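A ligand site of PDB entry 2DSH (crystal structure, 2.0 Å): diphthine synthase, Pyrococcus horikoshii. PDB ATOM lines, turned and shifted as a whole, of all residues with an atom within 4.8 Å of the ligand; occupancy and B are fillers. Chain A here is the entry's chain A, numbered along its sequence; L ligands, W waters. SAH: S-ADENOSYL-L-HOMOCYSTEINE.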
ATOM      1  N   LEU A  10      -4.950  17.921  26.431  1.00  0.00           N
ATOM      2  CA  LEU A  10      -4.002  17.445  25.435  1.00  0.00           C
ATOM      3  C   LEU A  10      -2.598  16.981  25.766  1.00  0.00           C
ATOM      4  O   LEU A  10      -2.165  15.917  25.318  1.00  0.00           O
ATOM      5  CB  LEU A  10      -3.865  18.520  24.362  1.00  0.00           C
ATOM      6  CG  LEU A  10      -5.123  18.970  23.632  1.00  0.00           C
ATOM      7  CD1 LEU A  10      -4.860  20.273  22.908  1.00  0.00           C
ATOM      8  CD2 LEU A  10      -5.570  17.882  22.683  1.00  0.00           C
ATOM      9  N   TYR A  11      -1.866  17.778  26.543  1.00  0.00           N
ATOM     10  CA  TYR A  11      -0.456  17.512  26.775  1.00  0.00           C
ATOM     11  C   TYR A  11       0.073  17.445  28.204  1.00  0.00           C
ATOM     12  O   TYR A  11       0.778  16.494  28.563  1.00  0.00           O
ATOM     13  CB  TYR A  11       0.322  18.557  25.965  1.00  0.00           C
ATOM     14  CG  TYR A  11       1.815  18.418  25.941  1.00  0.00           C
ATOM     15  CD1 TYR A  11       2.429  17.360  25.271  1.00  0.00           C
ATOM     16  CD2 TYR A  11       2.620  19.388  26.544  1.00  0.00           C
ATOM     17  CE1 TYR A  11       3.832  17.270  25.201  1.00  0.00           C
ATOM     18  CE2 TYR A  11       4.010  19.302  26.479  1.00  0.00           C
ATOM     19  CZ  TYR A  11       4.605  18.255  25.812  1.00  0.00           C
ATOM     20  OH  TYR A  11       5.969  18.187  25.750  1.00  0.00           O
ATOM     21  N   THR A  36      -6.391   5.587  27.189  1.00  0.00           N
ATOM     22  CA  THR A  36      -7.080   6.043  25.984  1.00  0.00           C
ATOM     23  C   THR A  36      -6.248   7.013  25.165  1.00  0.00           C
ATOM     24  O   THR A  36      -6.491   7.211  23.978  1.00  0.00           O
ATOM     25  CB  THR A  36      -8.436   6.722  26.312  1.00  0.00           C
ATOM     26  OG1 THR A  36      -8.224   7.796  27.230  1.00  0.00           O
ATOM     27  CG2 THR A  36      -9.406   5.706  26.910  1.00  0.00           C
ATOM     28  N   SER A  37      -5.269   7.637  25.809  1.00  0.00           N
ATOM     29  CA  SER A  37      -4.413   8.583  25.109  1.00  0.00           C
ATOM     30  C   SER A  37      -3.125   8.830  25.883  1.00  0.00           C
ATOM     31  O   SER A  37      -2.983   8.385  27.019  1.00  0.00           O
ATOM     32  CB  SER A  37      -5.147   9.900  24.890  1.00  0.00           C
ATOM     33  OG  SER A  37      -4.380  10.780  24.085  1.00  0.00           O
ATOM     34  N   LEU A  38      -2.194   9.552  25.268  1.00  0.00           N
ATOM     35  CA  LEU A  38      -0.936   9.855  25.905  1.00  0.00           C
ATOM     36  C   LEU A  38      -0.748  11.334  26.181  1.00  0.00           C
ATOM     37  O   LEU A  38      -0.846  12.166  25.273  1.00  0.00           O
ATOM     38  CB  LEU A  38       0.239   9.365  25.039  1.00  0.00           C
ATOM     39  CG  LEU A  38       1.651   9.736  25.484  1.00  0.00           C
ATOM     40  CD1 LEU A  38       1.974   9.097  26.837  1.00  0.00           C
ATOM     41  CD2 LEU A  38       2.647   9.277  24.437  1.00  0.00           C
ATOM     42  N   PRO A  85      -7.374  11.582  29.841  1.00  0.00           N
ATOM     43  CA  PRO A  85      -6.611  12.506  28.998  1.00  0.00           C
ATOM     44  C   PRO A  85      -7.596  13.165  28.039  1.00  0.00           C
ATOM     45  O   PRO A  85      -8.700  12.632  27.837  1.00  0.00           O
ATOM     46  CB  PRO A  85      -5.644  11.580  28.258  1.00  0.00           C
ATOM     47  CG  PRO A  85      -5.501  10.395  29.179  1.00  0.00           C
ATOM     48  CD  PRO A  85      -6.912  10.197  29.667  1.00  0.00           C
ATOM     49  N   GLY A  86      -7.220  14.299  27.462  1.00  0.00           N
ATOM     50  CA  GLY A  86      -8.094  14.999  26.519  1.00  0.00           C
ATOM     51  C   GLY A  86      -9.498  15.183  27.065  1.00  0.00           C
ATOM     52  O   GLY A  86      -9.659  15.512  28.238  1.00  0.00           O
ATOM     53  N   ASP A  87     -10.510  14.993  26.220  1.00  0.00           N
ATOM     54  CA  ASP A  87     -11.901  15.102  26.649  1.00  0.00           C
ATOM     55  C   ASP A  87     -12.365  13.682  26.972  1.00  0.00           C
ATOM     56  O   ASP A  87     -12.176  12.763  26.177  1.00  0.00           O
ATOM     57  CB  ASP A  87     -12.770  15.712  25.539  1.00  0.00           C
ATOM     58  CG  ASP A  87     -14.213  15.865  25.944  1.00  0.00           C
ATOM     59  OD1 ASP A  87     -14.897  14.834  26.159  1.00  0.00           O
ATOM     60  OD2 ASP A  87     -14.682  17.025  26.053  1.00  0.00           O
ATOM     61  N   VAL A  90     -14.540  11.766  24.111  1.00  0.00           N
ATOM     62  CA  VAL A  90     -14.152  11.831  22.709  1.00  0.00           C
ATOM     63  C   VAL A  90     -13.237  10.667  22.343  1.00  0.00           C
ATOM     64  O   VAL A  90     -12.153  10.527  22.897  1.00  0.00           O
ATOM     65  CB  VAL A  90     -13.420  13.155  22.376  1.00  0.00           C
ATOM     66  CG1 VAL A  90     -12.888  13.110  20.937  1.00  0.00           C
ATOM     67  CG2 VAL A  90     -14.365  14.341  22.550  1.00  0.00           C
ATOM     68  N   ALA A  91     -13.689   9.825  21.412  1.00  0.00           N
ATOM     69  CA  ALA A  91     -12.910   8.679  20.966  1.00  0.00           C
ATOM     70  C   ALA A  91     -12.596   7.710  22.100  1.00  0.00           C
ATOM     71  O   ALA A  91     -11.511   7.136  22.169  1.00  0.00           O
ATOM     72  CB  ALA A  91     -11.604   9.151  20.300  1.00  0.00           C
ATOM     73  N   THR A  92     -13.545   7.571  23.012  1.00  0.00           N
ATOM     74  CA  THR A  92     -13.427   6.648  24.135  1.00  0.00           C
ATOM     75  C   THR A  92     -14.813   6.034  24.205  1.00  0.00           C
ATOM     76  O   THR A  92     -15.723   6.456  23.482  1.00  0.00           O
ATOM     77  CB  THR A  92     -13.136   7.363  25.481  1.00  0.00           C
ATOM     78  OG1 THR A  92     -14.312   8.054  25.923  1.00  0.00           O
ATOM     79  CG2 THR A  92     -11.988   8.353  25.322  1.00  0.00           C
ATOM     80  N   PRO A 114      -9.624  20.403  26.495  1.00  0.00           N
ATOM     81  CA  PRO A 114      -9.187  20.443  25.095  1.00  0.00           C
ATOM     82  C   PRO A 114      -9.065  19.026  24.531  1.00  0.00           C
ATOM     83  O   PRO A 114      -8.530  18.143  25.189  1.00  0.00           O
ATOM     84  CB  PRO A 114      -7.831  21.148  25.167  1.00  0.00           C
ATOM     85  CG  PRO A 114      -7.963  22.014  26.367  1.00  0.00           C
ATOM     86  CD  PRO A 114      -8.678  21.142  27.359  1.00  0.00           C
ATOM     87  N   SER A 115      -9.559  18.831  23.311  1.00  0.00           N
ATOM     88  CA  SER A 115      -9.532  17.530  22.662  1.00  0.00           C
ATOM     89  C   SER A 115      -8.780  17.593  21.334  1.00  0.00           C
ATOM     90  O   SER A 115      -8.838  18.599  20.634  1.00  0.00           O
ATOM     91  CB  SER A 115     -10.965  17.044  22.405  1.00  0.00           C
ATOM     92  OG  SER A 115     -10.985  15.834  21.673  1.00  0.00           O
ATOM     93  N   ILE A 116      -8.082  16.516  20.994  1.00  0.00           N
ATOM     94  CA  ILE A 116      -7.334  16.484  19.740  1.00  0.00           C
ATOM     95  C   ILE A 116      -8.322  16.637  18.577  1.00  0.00           C
ATOM     96  O   ILE A 116      -7.969  17.163  17.532  1.00  0.00           O
ATOM     97  CB  ILE A 116      -6.562  15.159  19.579  1.00  0.00           C
ATOM     98  CG1 ILE A 116      -5.631  15.245  18.371  1.00  0.00           C
ATOM     99  CG2 ILE A 116      -7.536  13.987  19.443  1.00  0.00           C
ATOM    100  CD1 ILE A 116      -4.577  16.335  18.487  1.00  0.00           C
ATOM    101  N   TYR A 117      -9.559  16.197  18.794  1.00  0.00           N
ATOM    102  CA  TYR A 117     -10.586  16.275  17.764  1.00  0.00           C
ATOM    103  C   TYR A 117     -10.802  17.711  17.288  1.00  0.00           C
ATOM    104  O   TYR A 117     -11.096  17.947  16.105  1.00  0.00           O
ATOM    105  CB  TYR A 117     -11.894  15.662  18.299  1.00  0.00           C
ATOM    106  CG  TYR A 117     -13.040  15.611  17.312  1.00  0.00           C
ATOM    107  CD1 TYR A 117     -12.967  14.832  16.142  1.00  0.00           C
ATOM    108  CD2 TYR A 117     -14.221  16.315  17.552  1.00  0.00           C
ATOM    109  CE1 TYR A 117     -14.051  14.770  15.244  1.00  0.00           C
ATOM    110  CE2 TYR A 117     -15.292  16.256  16.685  1.00  0.00           C
ATOM    111  CZ  TYR A 117     -15.210  15.487  15.531  1.00  0.00           C
ATOM    112  OH  TYR A 117     -16.291  15.448  14.683  1.00  0.00           O
ATOM    113  N   PHE A 165      -7.051   8.979  14.042  1.00  0.00           N
ATOM    114  CA  PHE A 165      -6.530   8.759  15.375  1.00  0.00           C
ATOM    115  C   PHE A 165      -5.523   7.634  15.180  1.00  0.00           C
ATOM    116  O   PHE A 165      -5.746   6.749  14.346  1.00  0.00           O
ATOM    117  CB  PHE A 165      -7.648   8.289  16.301  1.00  0.00           C
ATOM    118  CG  PHE A 165      -8.677   9.348  16.588  1.00  0.00           C
ATOM    119  CD1 PHE A 165      -8.418  10.367  17.502  1.00  0.00           C
ATOM    120  CD2 PHE A 165      -9.907   9.336  15.923  1.00  0.00           C
ATOM    121  CE1 PHE A 165      -9.366  11.368  17.754  1.00  0.00           C
ATOM    122  CE2 PHE A 165     -10.853  10.336  16.161  1.00  0.00           C
ATOM    123  CZ  PHE A 165     -10.584  11.352  17.084  1.00  0.00           C
ATOM    124  N   LEU A 166      -4.416   7.686  15.902  1.00  0.00           N
ATOM    125  CA  LEU A 166      -3.404   6.643  15.784  1.00  0.00           C
ATOM    126  C   LEU A 166      -3.470   5.697  16.970  1.00  0.00           C
ATOM    127  O   LEU A 166      -3.791   6.094  18.086  1.00  0.00           O
ATOM    128  CB  LEU A 166      -2.010   7.279  15.656  1.00  0.00           C
ATOM    129  CG  LEU A 166      -1.865   8.192  14.434  1.00  0.00           C
ATOM    130  CD1 LEU A 166      -0.394   8.509  14.202  1.00  0.00           C
ATOM    131  CD2 LEU A 166      -2.457   7.509  13.195  1.00  0.00           C
ATOM    132  N   ASP A 167      -3.173   4.423  16.716  1.00  0.00           N
ATOM    133  CA  ASP A 167      -3.262   3.407  17.750  1.00  0.00           C
ATOM    134  C   ASP A 167      -2.342   3.595  18.947  1.00  0.00           C
ATOM    135  O   ASP A 167      -1.318   4.289  18.871  1.00  0.00           O
ATOM    136  CB  ASP A 167      -3.021   2.024  17.125  1.00  0.00           C
ATOM    137  CG  ASP A 167      -3.560   0.897  17.984  1.00  0.00           C
ATOM    138  OD1 ASP A 167      -4.458   1.151  18.818  1.00  0.00           O
ATOM    139  OD2 ASP A 167      -3.098  -0.243  17.801  1.00  0.00           O
ATOM    140  N   ILE A 168      -2.737   3.007  20.066  1.00  0.00           N
ATOM    141  CA  ILE A 168      -1.965   3.080  21.300  1.00  0.00           C
ATOM    142  C   ILE A 168      -2.154   1.816  22.127  1.00  0.00           C
ATOM    143  O   ILE A 168      -3.265   1.295  22.261  1.00  0.00           O
ATOM    144  CB  ILE A 168      -2.377   4.309  22.154  1.00  0.00           C
ATOM    145  CG1 ILE A 168      -1.697   4.226  23.522  1.00  0.00           C
ATOM    146  CG2 ILE A 168      -3.892   4.363  22.322  1.00  0.00           C
ATOM    147  CD1 ILE A 168      -2.016   5.389  24.458  1.00  0.00           C
ATOM    148  N   LEU A 206       0.317  16.222  13.006  1.00  0.00           N
ATOM    149  CA  LEU A 206       0.249  17.083  14.174  1.00  0.00           C
ATOM    150  C   LEU A 206       0.772  16.218  15.310  1.00  0.00           C
ATOM    151  O   LEU A 206       0.191  15.183  15.613  1.00  0.00           O
ATOM    152  CB  LEU A 206      -1.200  17.525  14.467  1.00  0.00           C
ATOM    153  CG  LEU A 206      -1.401  18.373  15.742  1.00  0.00           C
ATOM    154  CD1 LEU A 206      -0.467  19.586  15.705  1.00  0.00           C
ATOM    155  CD2 LEU A 206      -2.863  18.825  15.854  1.00  0.00           C
ATOM    156  N   ALA A 207       1.865  16.644  15.923  1.00  0.00           N
ATOM    157  CA  ALA A 207       2.445  15.872  17.021  1.00  0.00           C
ATOM    158  C   ALA A 207       2.492  16.689  18.295  1.00  0.00           C
ATOM    159  O   ALA A 207       2.906  17.858  18.275  1.00  0.00           O
ATOM    160  CB  ALA A 207       3.856  15.411  16.644  1.00  0.00           C
ATOM    161  N   ARG A 208       2.068  16.086  19.389  1.00  0.00           N
ATOM    162  CA  ARG A 208       2.059  16.732  20.697  1.00  0.00           C
ATOM    163  C   ARG A 208       1.252  18.031  20.724  1.00  0.00           C
ATOM    164  O   ARG A 208       1.720  19.057  21.206  1.00  0.00           O
ATOM    165  CB  ARG A 208       3.502  16.987  21.158  1.00  0.00           C
ATOM    166  CG  ARG A 208       4.384  15.728  21.155  1.00  0.00           C
ATOM    167  CD  ARG A 208       5.809  16.054  21.582  1.00  0.00           C
ATOM    168  NE  ARG A 208       6.367  17.128  20.772  1.00  0.00           N
ATOM    169  CZ  ARG A 208       6.681  17.009  19.487  1.00  0.00           C
ATOM    170  NH1 ARG A 208       6.501  15.853  18.849  1.00  0.00           N
ATOM    171  NH2 ARG A 208       7.131  18.058  18.818  1.00  0.00           N
ATOM    172  N   ALA A 209       0.035  17.973  20.185  1.00  0.00           N
ATOM    173  CA  ALA A 209      -0.832  19.145  20.207  1.00  0.00           C
ATOM    174  C   ALA A 209      -1.000  19.469  21.687  1.00  0.00           C
ATOM    175  O   ALA A 209      -0.959  18.562  22.517  1.00  0.00           O
ATOM    176  CB  ALA A 209      -2.188  18.826  19.569  1.00  0.00           C
ATOM    177  N   GLY A 210      -1.180  20.735  22.026  1.00  0.00           N
ATOM    178  CA  GLY A 210      -1.338  21.092  23.428  1.00  0.00           C
ATOM    179  C   GLY A 210      -0.045  21.656  23.974  1.00  0.00           C
ATOM    180  O   GLY A 210      -0.052  22.484  24.881  1.00  0.00           O
ATOM    181  N   PRO A 233       2.275  11.785  21.450  1.00  0.00           N
ATOM    182  CA  PRO A 233       1.391  11.168  20.462  1.00  0.00           C
ATOM    183  C   PRO A 233       1.349  11.922  19.129  1.00  0.00           C
ATOM    184  O   PRO A 233       1.650  13.109  19.069  1.00  0.00           O
ATOM    185  CB  PRO A 233       0.040  11.162  21.175  1.00  0.00           C
ATOM    186  CG  PRO A 233       0.085  12.473  21.921  1.00  0.00           C
ATOM    187  CD  PRO A 233       1.507  12.542  22.458  1.00  0.00           C
ATOM    188  N   HIS A 234       0.972  11.198  18.071  1.00  0.00           N
ATOM    189  CA  HIS A 234       0.866  11.797  16.740  1.00  0.00           C
ATOM    190  C   HIS A 234      -0.546  11.569  16.219  1.00  0.00           C
ATOM    191  O   HIS A 234      -1.235  10.646  16.629  1.00  0.00           O
ATOM    192  CB  HIS A 234       1.809  11.118  15.729  1.00  0.00           C
ATOM    193  CG  HIS A 234       3.267  11.316  16.009  1.00  0.00           C
ATOM    194  ND1 HIS A 234       4.244  10.849  15.160  1.00  0.00           N
ATOM    195  CD2 HIS A 234       3.912  11.926  17.029  1.00  0.00           C
ATOM    196  CE1 HIS A 234       5.438  11.165  15.643  1.00  0.00           C
ATOM    197  NE2 HIS A 234       5.263  11.816  16.780  1.00  0.00           N
ATOM    198  N   ILE A 235      -0.957  12.433  15.309  1.00  0.00           N
ATOM    199  CA  ILE A 235      -2.245  12.298  14.660  1.00  0.00           C
ATOM    200  C   ILE A 235      -1.946  12.513  13.188  1.00  0.00           C
ATOM    201  O   ILE A 235      -1.093  13.320  12.837  1.00  0.00           O
ATOM    202  CB  ILE A 235      -3.274  13.355  15.170  1.00  0.00           C
ATOM    203  CG1 ILE A 235      -4.688  12.840  14.960  1.00  0.00           C
ATOM    204  CG2 ILE A 235      -3.107  14.666  14.416  1.00  0.00           C
ATOM    205  CD1 ILE A 235      -5.076  11.749  15.921  1.00  0.00           C
HETATM  206  N   SAH L   1     -10.298  11.676  24.474  1.00  0.00           N
HETATM  207  CA  SAH L   1      -9.006  11.990  23.718  1.00  0.00           C
HETATM  208  CB  SAH L   1      -8.671  11.136  22.529  1.00  0.00           C
HETATM  209  CG  SAH L   1      -8.553   9.632  22.698  1.00  0.00           C
HETATM  210  SD  SAH L   1      -7.856   8.969  21.123  1.00  0.00           S
HETATM  211  C   SAH L   1      -9.081  13.525  23.296  1.00  0.00           C
HETATM  212  O   SAH L   1     -10.098  14.180  23.608  1.00  0.00           O
HETATM  213  OXT SAH L   1      -8.063  14.015  22.661  1.00  0.00           O
HETATM  214  C5' SAH L   1      -6.145   9.111  21.467  1.00  0.00           C
HETATM  215  C4' SAH L   1      -5.357   9.331  20.125  1.00  0.00           C
HETATM  216  O4' SAH L   1      -5.623  10.679  19.679  1.00  0.00           O
HETATM  217  C3' SAH L   1      -3.876   9.195  20.248  1.00  0.00           C
HETATM  218  O3' SAH L   1      -3.468   7.849  20.029  1.00  0.00           O
HETATM  219  C2' SAH L   1      -3.358  10.222  19.204  1.00  0.00           C
HETATM  220  O2' SAH L   1      -3.274   9.651  17.899  1.00  0.00           O
HETATM  221  C1' SAH L   1      -4.356  11.393  19.313  1.00  0.00           C
HETATM  222  N9  SAH L   1      -4.028  12.315  20.249  1.00  0.00           N
HETATM  223  C8  SAH L   1      -4.434  12.597  21.548  1.00  0.00           C
HETATM  224  N7  SAH L   1      -3.847  13.613  22.100  1.00  0.00           N
HETATM  225  C5  SAH L   1      -2.941  14.093  21.103  1.00  0.00           C
HETATM  226  C6  SAH L   1      -2.005  15.198  21.106  1.00  0.00           C
HETATM  227  N6  SAH L   1      -1.827  16.017  22.150  1.00  0.00           N
HETATM  228  N1  SAH L   1      -1.298  15.356  19.938  1.00  0.00           N
HETATM  229  C2  SAH L   1      -1.445  14.541  18.849  1.00  0.00           C
HETATM  230  N3  SAH L   1      -2.328  13.475  18.817  1.00  0.00           N
HETATM  231  C4  SAH L   1      -3.033  13.317  19.971  1.00  0.00           C
HETATM  232  O   HOH W   1      -3.911  12.936  25.384  1.00  0.00           O
HETATM  233  O   HOH W   2      -8.810  10.202  26.119  1.00  0.00           O
HETATM  234  O   HOH W   3      -0.852   6.990  20.092  1.00  0.00           O
HETATM  235  O   HOH W   4      -5.724  14.326  24.349  1.00  0.00           O
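The backbone carbonyl oxygen of Thr 36 sits close to a sulfur (SD) of the ligand.
OG of Ser 37 touches C8 of the ligand (3.1 Å).
Pro 85 touches the ligand (O to N, 3.8 Å).
Gly 86 touches the ligand (CA to O, 3.6 Å).
Ala 91 touches the ligand.
CG2 of Thr 92 touches N of the ligand, at 3.8 Å.
Phe 165 touches the ligand (CD1 to O4', 3.6 Å).
Leu 206 touches the ligand.
Pro 233 touches the ligand.
Ile 235 touches the ligand.
Hydrophobic or aromatic side chains that line the ligand: Leu 10, Val 90, Ala 91, Ile 116, Phe 165, Leu 166, Ala 209, Pro 233 and Ile 235.
Within 4 Å of the ligand: Leu 10, Thr 36, Ser 37, Pro 85, Gly 86, Asp 87, Val 90, Ala 91, Thr 92, Ser 115, Ile 116, Phe 165, Leu 166, Leu 206, Arg 208, Ala 209, Pro 233, His 234 and Ile 235.
Water W2 lies within hydrogen-bond range of N of the ligand (2.7 Å), OG1 of Thr 36 (2.7 Å) and O of Pro 85 (3.0 Å).
Water W3 bridges O3' of the ligand (2.8 Å) and O of Asp 167 (3.0 Å).
Water W4 bridges an oxygen (OXT) of the ligand (2.9 Å) and the backbone NH of Gly 86 (3.5 Å).
O3' of the ligand sits at hydrogen-bond distance from O of Leu 166 (2.6 Å).
An oxygen (OXT) of the ligand lies within hydrogen-bond range of the backbone NH (N) of Ile 116.
A nitrogen (N6) of the ligand sits at hydrogen-bond distance from the backbone carbonyl oxygen (O) of Ala 209 (2.7 Å).
The backbone NH (N) of Arg 208 is in hydrogen-bond range of a nitrogen (N1) of the ligand (3.5 Å).
An oxygen (O) of the ligand lies within hydrogen-bond range of the side-chain hydroxyl of Ser 115 (2.7 Å).
O of Leu 10 sits at hydrogen-bond distance from N6 of the ligand.
The backbone carbonyl oxygen (O) of His 234 sits at hydrogen-bond distance from an oxygen (O2') of the ligand (2.6 Å).
O of the ligand is in hydrogen-bond range of N of Asp 87, 2.8 Å away.
A nitrogen (N1) of the ligand lies within hydrogen-bond range of the backbone NH (N) of Ala 209 (2.9 Å).
The backbone carbonyl oxygen (O) of Asp 87 lies within hydrogen-bond range of a nitrogen (N) of the ligand, at 2.8 Å.
The backbone carbonyl oxygen of Val 90 is in hydrogen-bond range of a nitrogen (N) of the ligand, at 2.7 Å.
The backbone NH of Leu 166 is in hydrogen-bond range of an oxygen (O2') of the ligand (3.0 Å).
The backbone carbonyl oxygen (O) of Pro 233 lies within hydrogen-bond range of the backbone NH (N) of Arg 208 (3.0 Å).
N of Ile 235 is in hydrogen-bond range of O of Leu 206, 3.0 Å away.
The backbone NH (N) of Tyr 117 sits close to the side-chain hydroxyl (OG) of Ser 115, at 3.2 Å.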
